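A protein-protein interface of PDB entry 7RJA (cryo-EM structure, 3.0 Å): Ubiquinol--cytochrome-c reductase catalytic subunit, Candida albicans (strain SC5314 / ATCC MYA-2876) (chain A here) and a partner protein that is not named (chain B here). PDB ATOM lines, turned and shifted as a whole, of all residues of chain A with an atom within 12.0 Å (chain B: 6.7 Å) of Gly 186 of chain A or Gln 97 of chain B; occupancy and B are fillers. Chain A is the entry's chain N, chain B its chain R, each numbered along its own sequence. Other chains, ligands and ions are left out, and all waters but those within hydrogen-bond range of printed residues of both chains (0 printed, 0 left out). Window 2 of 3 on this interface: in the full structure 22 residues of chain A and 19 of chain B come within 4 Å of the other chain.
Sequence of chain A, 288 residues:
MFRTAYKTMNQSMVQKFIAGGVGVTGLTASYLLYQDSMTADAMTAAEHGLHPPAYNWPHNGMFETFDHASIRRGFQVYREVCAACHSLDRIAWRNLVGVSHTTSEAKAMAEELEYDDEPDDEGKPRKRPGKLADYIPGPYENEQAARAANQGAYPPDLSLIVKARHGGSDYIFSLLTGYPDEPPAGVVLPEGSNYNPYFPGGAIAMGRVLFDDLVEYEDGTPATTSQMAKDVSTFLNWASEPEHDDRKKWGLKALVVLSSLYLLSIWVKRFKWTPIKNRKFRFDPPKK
N of Gly 201 of chain A sits at hydrogen-bond distance from O of Ala 46 of chain A, at 3.0 Å.
The side-chain hydroxyl of Thr 94 of chain B sits at hydrogen-bond distance from the backbone carbonyl oxygen of Ile 90 of chain B (3.1 Å).
N of Ile 90 of chain B is in hydrogen-bond range of SG of Cys 111 of chain B (3.5 Å).
OE2 of Glu 109 of chain B lies within salt-bridge range of NH2 of Arg 92 of chain B.
OE1 of Glu 96 of chain B sits close to N of Glu 109 of chain B (3.4 Å).
The backbone carbonyl oxygen (O) of Ala 185 of chain A is in hydrogen-bond range of the backbone NH (N) of Cys 111 of chain B, at 3.0 Å.
Ile 112 of chain B touches Ala 46 of chain A.
CD1 of Ile 90 of chain B touches CB of Ala 185 of chain A (3.4 Å).
C of Ala 185 of chain A touches CG1 of Val 93 of chain B, 3.7 Å away.
Ala 185 of chain A touches Asp 110 of chain B.
CG1 of Val 93 of chain B touches CA of Gly 186 of chain A, at 3.5 Å.
Gly 186 of chain A touches Gln 97 of chain B.
Gly 186 of chain A touches Glu 109 of chain B (CA to O, 3.6 Å).
Gly 186 of chain A touches Asp 110 of chain B.
CG2 of Val 187 of chain A touches CD1 of Ile 112 of chain B (3.9 Å).
Tyr 195 of chain A touches Ile 112 of chain B.
Of the 17 printed residues of chain B, 7 touch a printed residue of chain A.
Printed residues of chain B that touch a printed residue of chain A: Ile 90, Val 93, Gln 97, Glu 109, Asp 110, Cys 111 and Ile 112.
Of the 15 printed residues of chain A, 5 touch a printed residue of chain B.
Among the printed residues, 11 pairs touch across the chains.
Among the printed residues, no Asp or Glu carboxylate lies within 4 Å of a Lys or Arg side-chain nitrogen of the other chain.
Printed residues of chain B within 4 Å of Ala 46 of chain A: Ile 112.
Of the printed residues of chain B, Ala 185 of chain A touches Ile 90, Val 93, Asp 110 and Cys 111.
Of chain B, only Val 93, Gln 97, Glu 109 and Asp 110 come within 4 Å of Gly 186 of chain A.
Gly 202 of chain A touches none of the printed residues of chain B.
Ile 90 of chain B touches just one residue of chain A: Ala 185 (3.4 Å).
Val 93 of chain B touches two residues of chain A.
No residue of chain A comes within 4 Å of Thr 94 of chain B.
No residue of chain A comes within 4 Å of Glu 96 of chain B.
Of chain A, only Gly 186 comes within 4 Å of Gln 97 of chain B.
Of the printed residues of chain A, Glu 109 of chain B touches Gly 186.
Of the printed residues of chain A, Asp 110 of chain B touches Ala 185 and Gly 186.
The nearest residue of chain B that does not touch Gly 186 of chain A is Tyr 102 of chain B (4.3 Å).
The nearest residue of chain A that does not touch Gln 97 of chain B is Ala 185 of chain A (4.9 Å).
The nearest printed residue of chain B that does not touch Val 187 of chain A is Asp 110 of chain B (4.1 Å).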
ATOM      1  N   ALA A  46      21.754  -9.292  -6.100  1.00  0.00           N
ATOM      2  CA  ALA A  46      20.322  -9.063  -5.937  1.00  0.00           C
ATOM      3  C   ALA A  46      19.539  -9.475  -7.178  1.00  0.00           C
ATOM      4  O   ALA A  46      18.523 -10.170  -7.072  1.00  0.00           O
ATOM      5  CB  ALA A  46      20.063  -7.595  -5.608  1.00  0.00           C
ATOM      6  N   PRO A 180      11.578 -11.408   4.828  1.00  0.00           N
ATOM      7  CA  PRO A 180      12.038 -10.915   6.125  1.00  0.00           C
ATOM      8  C   PRO A 180      11.048  -9.934   6.728  1.00  0.00           C
ATOM      9  O   PRO A 180      10.379  -9.174   6.025  1.00  0.00           O
ATOM     10  CB  PRO A 180      13.363 -10.230   5.783  1.00  0.00           C
ATOM     11  CG  PRO A 180      13.144  -9.708   4.415  1.00  0.00           C
ATOM     12  CD  PRO A 180      12.212 -10.673   3.719  1.00  0.00           C
ATOM     13  N   GLU A 182      11.582  -7.230   8.322  1.00  0.00           N
ATOM     14  CA  GLU A 182      11.973  -5.865   7.984  1.00  0.00           C
ATOM     15  C   GLU A 182      12.871  -5.921   6.756  1.00  0.00           C
ATOM     16  O   GLU A 182      13.940  -6.561   6.804  1.00  0.00           O
ATOM     17  CB  GLU A 182      12.691  -5.192   9.155  1.00  0.00           C
ATOM     18  N   PRO A 183      12.502  -5.282   5.646  1.00  0.00           N
ATOM     19  CA  PRO A 183      13.366  -5.322   4.473  1.00  0.00           C
ATOM     20  C   PRO A 183      14.723  -4.740   4.794  1.00  0.00           C
ATOM     21  O   PRO A 183      14.848  -3.843   5.651  1.00  0.00           O
ATOM     22  CB  PRO A 183      12.612  -4.463   3.447  1.00  0.00           C
ATOM     23  CG  PRO A 183      11.221  -4.401   3.921  1.00  0.00           C
ATOM     24  CD  PRO A 183      11.266  -4.522   5.402  1.00  0.00           C
ATOM     25  N   PRO A 184      15.781  -5.219   4.140  1.00  0.00           N
ATOM     26  CA  PRO A 184      17.114  -4.681   4.421  1.00  0.00           C
ATOM     27  C   PRO A 184      17.150  -3.179   4.193  1.00  0.00           C
ATOM     28  O   PRO A 184      16.622  -2.668   3.204  1.00  0.00           O
ATOM     29  CB  PRO A 184      18.017  -5.430   3.436  1.00  0.00           C
ATOM     30  CG  PRO A 184      17.110  -5.872   2.348  1.00  0.00           C
ATOM     31  CD  PRO A 184      15.794  -6.153   3.002  1.00  0.00           C
ATOM     32  N   ALA A 185      17.789  -2.471   5.119  1.00  0.00           N
ATOM     33  CA  ALA A 185      17.756  -1.016   5.090  1.00  0.00           C
ATOM     34  C   ALA A 185      18.352  -0.490   3.793  1.00  0.00           C
ATOM     35  O   ALA A 185      19.339  -1.022   3.280  1.00  0.00           O
ATOM     36  CB  ALA A 185      18.520  -0.446   6.284  1.00  0.00           C
ATOM     37  N   GLY A 186      17.736   0.564   3.258  1.00  0.00           N
ATOM     38  CA  GLY A 186      18.205   1.237   2.074  1.00  0.00           C
ATOM     39  C   GLY A 186      17.469   0.853   0.806  1.00  0.00           C
ATOM     40  O   GLY A 186      17.530   1.595  -0.181  1.00  0.00           O
ATOM     41  N   VAL A 187      16.777  -0.279   0.807  1.00  0.00           N
ATOM     42  CA  VAL A 187      16.051  -0.725  -0.374  1.00  0.00           C
ATOM     43  C   VAL A 187      14.648  -0.139  -0.352  1.00  0.00           C
ATOM     44  O   VAL A 187      13.933  -0.229   0.653  1.00  0.00           O
ATOM     45  CB  VAL A 187      16.018  -2.262  -0.439  1.00  0.00           C
ATOM     46  CG1 VAL A 187      15.053  -2.819   0.595  1.00  0.00           C
ATOM     47  CG2 VAL A 187      15.642  -2.724  -1.838  1.00  0.00           C
ATOM     48  N   VAL A 188      14.251   0.473  -1.465  1.00  0.00           N
ATOM     49  CA  VAL A 188      12.929   1.067  -1.615  1.00  0.00           C
ATOM     50  C   VAL A 188      12.160   0.251  -2.644  1.00  0.00           C
ATOM     51  O   VAL A 188      12.611   0.092  -3.785  1.00  0.00           O
ATOM     52  CB  VAL A 188      13.014   2.546  -2.029  1.00  0.00           C
ATOM     53  CG1 VAL A 188      13.632   2.691  -3.412  1.00  0.00           C
ATOM     54  CG2 VAL A 188      11.636   3.188  -1.985  1.00  0.00           C
ATOM     55  N   LEU A 189      11.005  -0.264  -2.239  1.00  0.00           N
ATOM     56  CA  LEU A 189      10.217  -1.134  -3.096  1.00  0.00           C
ATOM     57  C   LEU A 189       9.142  -0.341  -3.826  1.00  0.00           C
ATOM     58  O   LEU A 189       8.511   0.540  -3.232  1.00  0.00           O
ATOM     59  CB  LEU A 189       9.547  -2.232  -2.273  1.00  0.00           C
ATOM     60  CG  LEU A 189      10.444  -2.956  -1.272  1.00  0.00           C
ATOM     61  CD1 LEU A 189       9.631  -3.965  -0.490  1.00  0.00           C
ATOM     62  CD2 LEU A 189      11.602  -3.632  -1.980  1.00  0.00           C
ATOM     63  N   PRO A 190       8.893  -0.620  -5.104  1.00  0.00           N
ATOM     64  CA  PRO A 190       7.763   0.025  -5.777  1.00  0.00           C
ATOM     65  C   PRO A 190       6.463  -0.295  -5.060  1.00  0.00           C
ATOM     66  O   PRO A 190       6.278  -1.392  -4.529  1.00  0.00           O
ATOM     67  CB  PRO A 190       7.794  -0.575  -7.187  1.00  0.00           C
ATOM     68  CG  PRO A 190       9.190  -1.052  -7.365  1.00  0.00           C
ATOM     69  CD  PRO A 190       9.630  -1.511  -6.014  1.00  0.00           C
ATOM     70  N   TYR A 195       9.440  -7.222  -0.447  1.00  0.00           N
ATOM     71  CA  TYR A 195      10.823  -7.659  -0.572  1.00  0.00           C
ATOM     72  C   TYR A 195      10.953  -9.142  -0.262  1.00  0.00           C
ATOM     73  O   TYR A 195      10.480  -9.614   0.776  1.00  0.00           O
ATOM     74  CB  TYR A 195      11.738  -6.865   0.354  1.00  0.00           C
ATOM     75  CG  TYR A 195      13.194  -7.187   0.124  1.00  0.00           C
ATOM     76  CD1 TYR A 195      13.890  -6.610  -0.922  1.00  0.00           C
ATOM     77  CD2 TYR A 195      13.862  -8.087   0.936  1.00  0.00           C
ATOM     78  CE1 TYR A 195      15.213  -6.907  -1.144  1.00  0.00           C
ATOM     79  CE2 TYR A 195      15.186  -8.390   0.721  1.00  0.00           C
ATOM     80  CZ  TYR A 195      15.856  -7.797  -0.321  1.00  0.00           C
ATOM     81  OH  TYR A 195      17.178  -8.093  -0.548  1.00  0.00           O
ATOM     82  N   GLY A 201      15.887  -9.669  -8.446  1.00  0.00           N
ATOM     83  CA  GLY A 201      15.644  -8.257  -8.287  1.00  0.00           C
ATOM     84  C   GLY A 201      15.249  -7.839  -6.888  1.00  0.00           C
ATOM     85  O   GLY A 201      15.344  -6.651  -6.561  1.00  0.00           O
ATOM     86  N   GLY A 202      14.810  -8.778  -6.053  1.00  0.00           N
ATOM     87  CA  GLY A 202      14.496  -8.490  -4.675  1.00  0.00           C
ATOM     88  C   GLY A 202      13.089  -8.006  -4.416  1.00  0.00           C
ATOM     89  O   GLY A 202      12.660  -8.009  -3.258  1.00  0.00           O
ATOM     90  N   ALA A 203      12.350  -7.596  -5.444  1.00  0.00           N
ATOM     91  CA  ALA A 203      10.998  -7.075  -5.281  1.00  0.00           C
ATOM     92  C   ALA A 203      10.018  -8.035  -5.933  1.00  0.00           C
ATOM     93  O   ALA A 203      10.064  -8.238  -7.150  1.00  0.00           O
ATOM     94  CB  ALA A 203      10.869  -5.680  -5.894  1.00  0.00           C
ATOM     95  N   ILE B  90      23.124  -1.558   8.629  1.00  0.00           N
ATOM     96  CA  ILE B  90      21.809  -0.976   8.883  1.00  0.00           C
ATOM     97  C   ILE B  90      21.968   0.389   9.534  1.00  0.00           C
ATOM     98  O   ILE B  90      21.318   1.369   9.144  1.00  0.00           O
ATOM     99  CB  ILE B  90      20.959  -1.914   9.758  1.00  0.00           C
ATOM    100  CG1 ILE B  90      20.692  -3.240   9.038  1.00  0.00           C
ATOM    101  CG2 ILE B  90      19.660  -1.230  10.152  1.00  0.00           C
ATOM    102  CD1 ILE B  90      19.616  -3.174   7.979  1.00  0.00           C
ATOM    103  N   ARG B  92      24.565   2.417   9.406  1.00  0.00           N
ATOM    104  CA  ARG B  92      25.139   3.379   8.470  1.00  0.00           C
ATOM    105  C   ARG B  92      24.096   3.872   7.475  1.00  0.00           C
ATOM    106  O   ARG B  92      24.058   5.062   7.141  1.00  0.00           O
ATOM    107  CB  ARG B  92      26.323   2.759   7.732  1.00  0.00           C
ATOM    108  CG  ARG B  92      27.047   3.736   6.818  1.00  0.00           C
ATOM    109  CD  ARG B  92      28.339   3.153   6.275  1.00  0.00           C
ATOM    110  NE  ARG B  92      28.098   2.003   5.411  1.00  0.00           N
ATOM    111  CZ  ARG B  92      28.039   0.746   5.829  1.00  0.00           C
ATOM    112  NH1 ARG B  92      28.221   0.427   7.101  1.00  0.00           N
ATOM    113  NH2 ARG B  92      27.794  -0.220   4.948  1.00  0.00           N
ATOM    114  N   VAL B  93      23.250   2.970   6.979  1.00  0.00           N
ATOM    115  CA  VAL B  93      22.242   3.370   6.005  1.00  0.00           C
ATOM    116  C   VAL B  93      21.204   4.271   6.655  1.00  0.00           C
ATOM    117  O   VAL B  93      20.715   5.224   6.036  1.00  0.00           O
ATOM    118  CB  VAL B  93      21.596   2.131   5.361  1.00  0.00           C
ATOM    119  CG1 VAL B  93      20.423   2.542   4.489  1.00  0.00           C
ATOM    120  CG2 VAL B  93      22.623   1.377   4.540  1.00  0.00           C
ATOM    121  N   THR B  94      20.847   3.994   7.910  1.00  0.00           N
ATOM    122  CA  THR B  94      19.952   4.905   8.615  1.00  0.00           C
ATOM    123  C   THR B  94      20.580   6.287   8.742  1.00  0.00           C
ATOM    124  O   THR B  94      19.919   7.303   8.491  1.00  0.00           O
ATOM    125  CB  THR B  94      19.606   4.344   9.992  1.00  0.00           C
ATOM    126  OG1 THR B  94      20.811   4.014  10.694  1.00  0.00           O
ATOM    127  CG2 THR B  94      18.733   3.104   9.857  1.00  0.00           C
ATOM    128  N   LYS B  95      21.863   6.345   9.103  1.00  0.00           N
ATOM    129  CA  LYS B  95      22.549   7.632   9.180  1.00  0.00           C
ATOM    130  C   LYS B  95      22.500   8.358   7.843  1.00  0.00           C
ATOM    131  O   LYS B  95      22.214   9.559   7.784  1.00  0.00           O
ATOM    132  CB  LYS B  95      23.998   7.437   9.627  1.00  0.00           C
ATOM    133  CG  LYS B  95      24.167   6.825  11.008  1.00  0.00           C
ATOM    134  CD  LYS B  95      23.571   7.693  12.107  1.00  0.00           C
ATOM    135  CE  LYS B  95      24.330   9.002  12.269  1.00  0.00           C
ATOM    136  NZ  LYS B  95      25.729   8.784  12.728  1.00  0.00           N
ATOM    137  N   GLU B  96      22.776   7.642   6.752  1.00  0.00           N
ATOM    138  CA  GLU B  96      22.694   8.269   5.437  1.00  0.00           C
ATOM    139  C   GLU B  96      21.297   8.805   5.168  1.00  0.00           C
ATOM    140  O   GLU B  96      21.148   9.901   4.616  1.00  0.00           O
ATOM    141  CB  GLU B  96      23.092   7.281   4.340  1.00  0.00           C
ATOM    142  CG  GLU B  96      24.572   6.967   4.284  1.00  0.00           C
ATOM    143  CD  GLU B  96      24.930   6.103   3.092  1.00  0.00           C
ATOM    144  OE1 GLU B  96      24.004   5.660   2.380  1.00  0.00           O
ATOM    145  OE2 GLU B  96      26.135   5.870   2.861  1.00  0.00           O
ATOM    146  N   GLN B  97      20.266   8.053   5.547  1.00  0.00           N
ATOM    147  CA  GLN B  97      18.900   8.525   5.367  1.00  0.00           C
ATOM    148  C   GLN B  97      18.581   9.732   6.236  1.00  0.00           C
ATOM    149  O   GLN B  97      17.673  10.496   5.892  1.00  0.00           O
ATOM    150  CB  GLN B  97      17.913   7.398   5.670  1.00  0.00           C
ATOM    151  CG  GLN B  97      17.920   6.281   4.644  1.00  0.00           C
ATOM    152  CD  GLN B  97      16.939   5.181   4.981  1.00  0.00           C
ATOM    153  OE1 GLN B  97      16.292   5.209   6.028  1.00  0.00           O
ATOM    154  NE2 GLN B  97      16.820   4.202   4.093  1.00  0.00           N
ATOM    155  N   GLU B  98      19.300   9.927   7.342  1.00  0.00           N
ATOM    156  CA  GLU B  98      19.058  11.098   8.178  1.00  0.00           C
ATOM    157  C   GLU B  98      19.395  12.401   7.461  1.00  0.00           C
ATOM    158  O   GLU B  98      18.674  13.392   7.620  1.00  0.00           O
ATOM    159  CB  GLU B  98      19.871  11.005   9.471  1.00  0.00           C
ATOM    160  CG  GLU B  98      19.452   9.873  10.391  1.00  0.00           C
ATOM    161  CD  GLU B  98      18.062  10.069  10.960  1.00  0.00           C
ATOM    162  OE1 GLU B  98      17.660  11.233  11.166  1.00  0.00           O
ATOM    163  OE2 GLU B  98      17.370   9.057  11.199  1.00  0.00           O
ATOM    164  N   GLU B  99      20.468  12.421   6.680  1.00  0.00           N
ATOM    165  CA  GLU B  99      20.919  13.663   6.070  1.00  0.00           C
ATOM    166  C   GLU B  99      19.854  14.172   5.098  1.00  0.00           C
ATOM    167  O   GLU B  99      19.361  13.405   4.262  1.00  0.00           O
ATOM    168  CB  GLU B  99      22.249  13.433   5.347  1.00  0.00           C
ATOM    169  CG  GLU B  99      22.957  14.692   4.869  1.00  0.00           C
ATOM    170  CD  GLU B  99      22.447  15.196   3.534  1.00  0.00           C
ATOM    171  OE1 GLU B  99      21.978  14.373   2.720  1.00  0.00           O
ATOM    172  OE2 GLU B  99      22.517  16.421   3.299  1.00  0.00           O
ATOM    173  N   PRO B 100      19.473  15.453   5.174  1.00  0.00           N
ATOM    174  CA  PRO B 100      18.301  15.915   4.409  1.00  0.00           C
ATOM    175  C   PRO B 100      18.434  15.766   2.903  1.00  0.00           C
ATOM    176  O   PRO B 100      17.420  15.526   2.236  1.00  0.00           O
ATOM    177  CB  PRO B 100      18.180  17.390   4.810  1.00  0.00           C
ATOM    178  CG  PRO B 100      19.546  17.776   5.242  1.00  0.00           C
ATOM    179  CD  PRO B 100      20.116  16.560   5.901  1.00  0.00           C
ATOM    180  N   TYR B 102      19.417  13.374   1.282  1.00  0.00           N
ATOM    181  CA  TYR B 102      19.475  11.960   0.931  1.00  0.00           C
ATOM    182  C   TYR B 102      18.818  11.696  -0.418  1.00  0.00           C
ATOM    183  O   TYR B 102      19.376  10.989  -1.264  1.00  0.00           O
ATOM    184  CB  TYR B 102      18.804  11.130   2.025  1.00  0.00           C
ATOM    185  CG  TYR B 102      18.797   9.650   1.742  1.00  0.00           C
ATOM    186  CD1 TYR B 102      19.933   8.880   1.939  1.00  0.00           C
ATOM    187  CD2 TYR B 102      17.653   9.022   1.277  1.00  0.00           C
ATOM    188  CE1 TYR B 102      19.928   7.526   1.680  1.00  0.00           C
ATOM    189  CE2 TYR B 102      17.637   7.670   1.016  1.00  0.00           C
ATOM    190  CZ  TYR B 102      18.778   6.926   1.218  1.00  0.00           C
ATOM    191  OH  TYR B 102      18.766   5.575   0.959  1.00  0.00           O
ATOM    192  N   LYS B 105      20.996  12.156  -3.411  1.00  0.00           N
ATOM    193  CA  LYS B 105      22.180  11.334  -3.622  1.00  0.00           C
ATOM    194  C   LYS B 105      21.975  10.377  -4.787  1.00  0.00           C
ATOM    195  O   LYS B 105      20.938   9.717  -4.894  1.00  0.00           O
ATOM    196  CB  LYS B 105      22.509  10.553  -2.351  1.00  0.00           C
ATOM    197  CG  LYS B 105      22.969  11.419  -1.196  1.00  0.00           C
ATOM    198  CD  LYS B 105      23.307  10.581   0.023  1.00  0.00           C
ATOM    199  CE  LYS B 105      23.748  11.448   1.187  1.00  0.00           C
ATOM    200  NZ  LYS B 105      24.072  10.643   2.396  1.00  0.00           N
ATOM    201  N   LYS B 108      22.493   5.789  -3.273  1.00  0.00           N
ATOM    202  CA  LYS B 108      21.856   5.635  -1.968  1.00  0.00           C
ATOM    203  C   LYS B 108      22.157   4.222  -1.487  1.00  0.00           C
ATOM    204  O   LYS B 108      21.580   3.249  -1.980  1.00  0.00           O
ATOM    205  CB  LYS B 108      20.359   5.902  -2.067  1.00  0.00           C
ATOM    206  CG  LYS B 108      20.005   7.377  -1.979  1.00  0.00           C
ATOM    207  CD  LYS B 108      18.512   7.609  -2.112  1.00  0.00           C
ATOM    208  CE  LYS B 108      18.114   7.842  -3.559  1.00  0.00           C
ATOM    209  NZ  LYS B 108      18.645   9.132  -4.082  1.00  0.00           N
ATOM    210  N   GLU B 109      23.067   4.111  -0.523  1.00  0.00           N
ATOM    211  CA  GLU B 109      23.574   2.810  -0.120  1.00  0.00           C
ATOM    212  C   GLU B 109      22.454   1.938   0.431  1.00  0.00           C
ATOM    213  O   GLU B 109      21.446   2.421   0.950  1.00  0.00           O
ATOM    214  CB  GLU B 109      24.674   2.965   0.928  1.00  0.00           C
ATOM    215  CG  GLU B 109      25.401   1.671   1.252  1.00  0.00           C
ATOM    216  CD  GLU B 109      26.621   1.888   2.122  1.00  0.00           C
ATOM    217  OE1 GLU B 109      27.285   2.933   1.966  1.00  0.00           O
ATOM    218  OE2 GLU B 109      26.913   1.017   2.968  1.00  0.00           O
ATOM    219  N   ASP B 110      22.646   0.629   0.304  1.00  0.00           N
ATOM    220  CA  ASP B 110      21.693  -0.347   0.805  1.00  0.00           C
ATOM    221  C   ASP B 110      22.456  -1.565   1.299  1.00  0.00           C
ATOM    222  O   ASP B 110      23.561  -1.860   0.836  1.00  0.00           O
ATOM    223  CB  ASP B 110      20.673  -0.732  -0.271  1.00  0.00           C
ATOM    224  CG  ASP B 110      21.315  -1.400  -1.469  1.00  0.00           C
ATOM    225  OD1 ASP B 110      22.557  -1.532  -1.491  1.00  0.00           O
ATOM    226  OD2 ASP B 110      20.577  -1.784  -2.400  1.00  0.00           O
ATOM    227  N   CYS B 111      21.855  -2.273   2.253  1.00  0.00           N
ATOM    228  CA  CYS B 111      22.494  -3.404   2.910  1.00  0.00           C
ATOM    229  C   CYS B 111      22.067  -4.735   2.312  1.00  0.00           C
ATOM    230  O   CYS B 111      21.993  -5.742   3.024  1.00  0.00           O
ATOM    231  CB  CYS B 111      22.192  -3.376   4.405  1.00  0.00           C
ATOM    232  SG  CYS B 111      22.788  -1.887   5.197  1.00  0.00           S
ATOM    233  N   ILE B 112      21.785  -4.762   1.010  1.00  0.00           N
ATOM    234  CA  ILE B 112      21.372  -6.007   0.376  1.00  0.00           C
ATOM    235  C   ILE B 112      22.519  -7.007   0.371  1.00  0.00           C
ATOM    236  O   ILE B 112      22.306  -8.212   0.522  1.00  0.00           O
ATOM    237  CB  ILE B 112      20.848  -5.738  -1.045  1.00  0.00           C
ATOM    238  CG1 ILE B 112      19.653  -4.787  -0.997  1.00  0.00           C
ATOM    239  CG2 ILE B 112      20.445  -7.039  -1.709  1.00  0.00           C
ATOM    240  CD1 ILE B 112      19.200  -4.314  -2.356  1.00  0.00           C
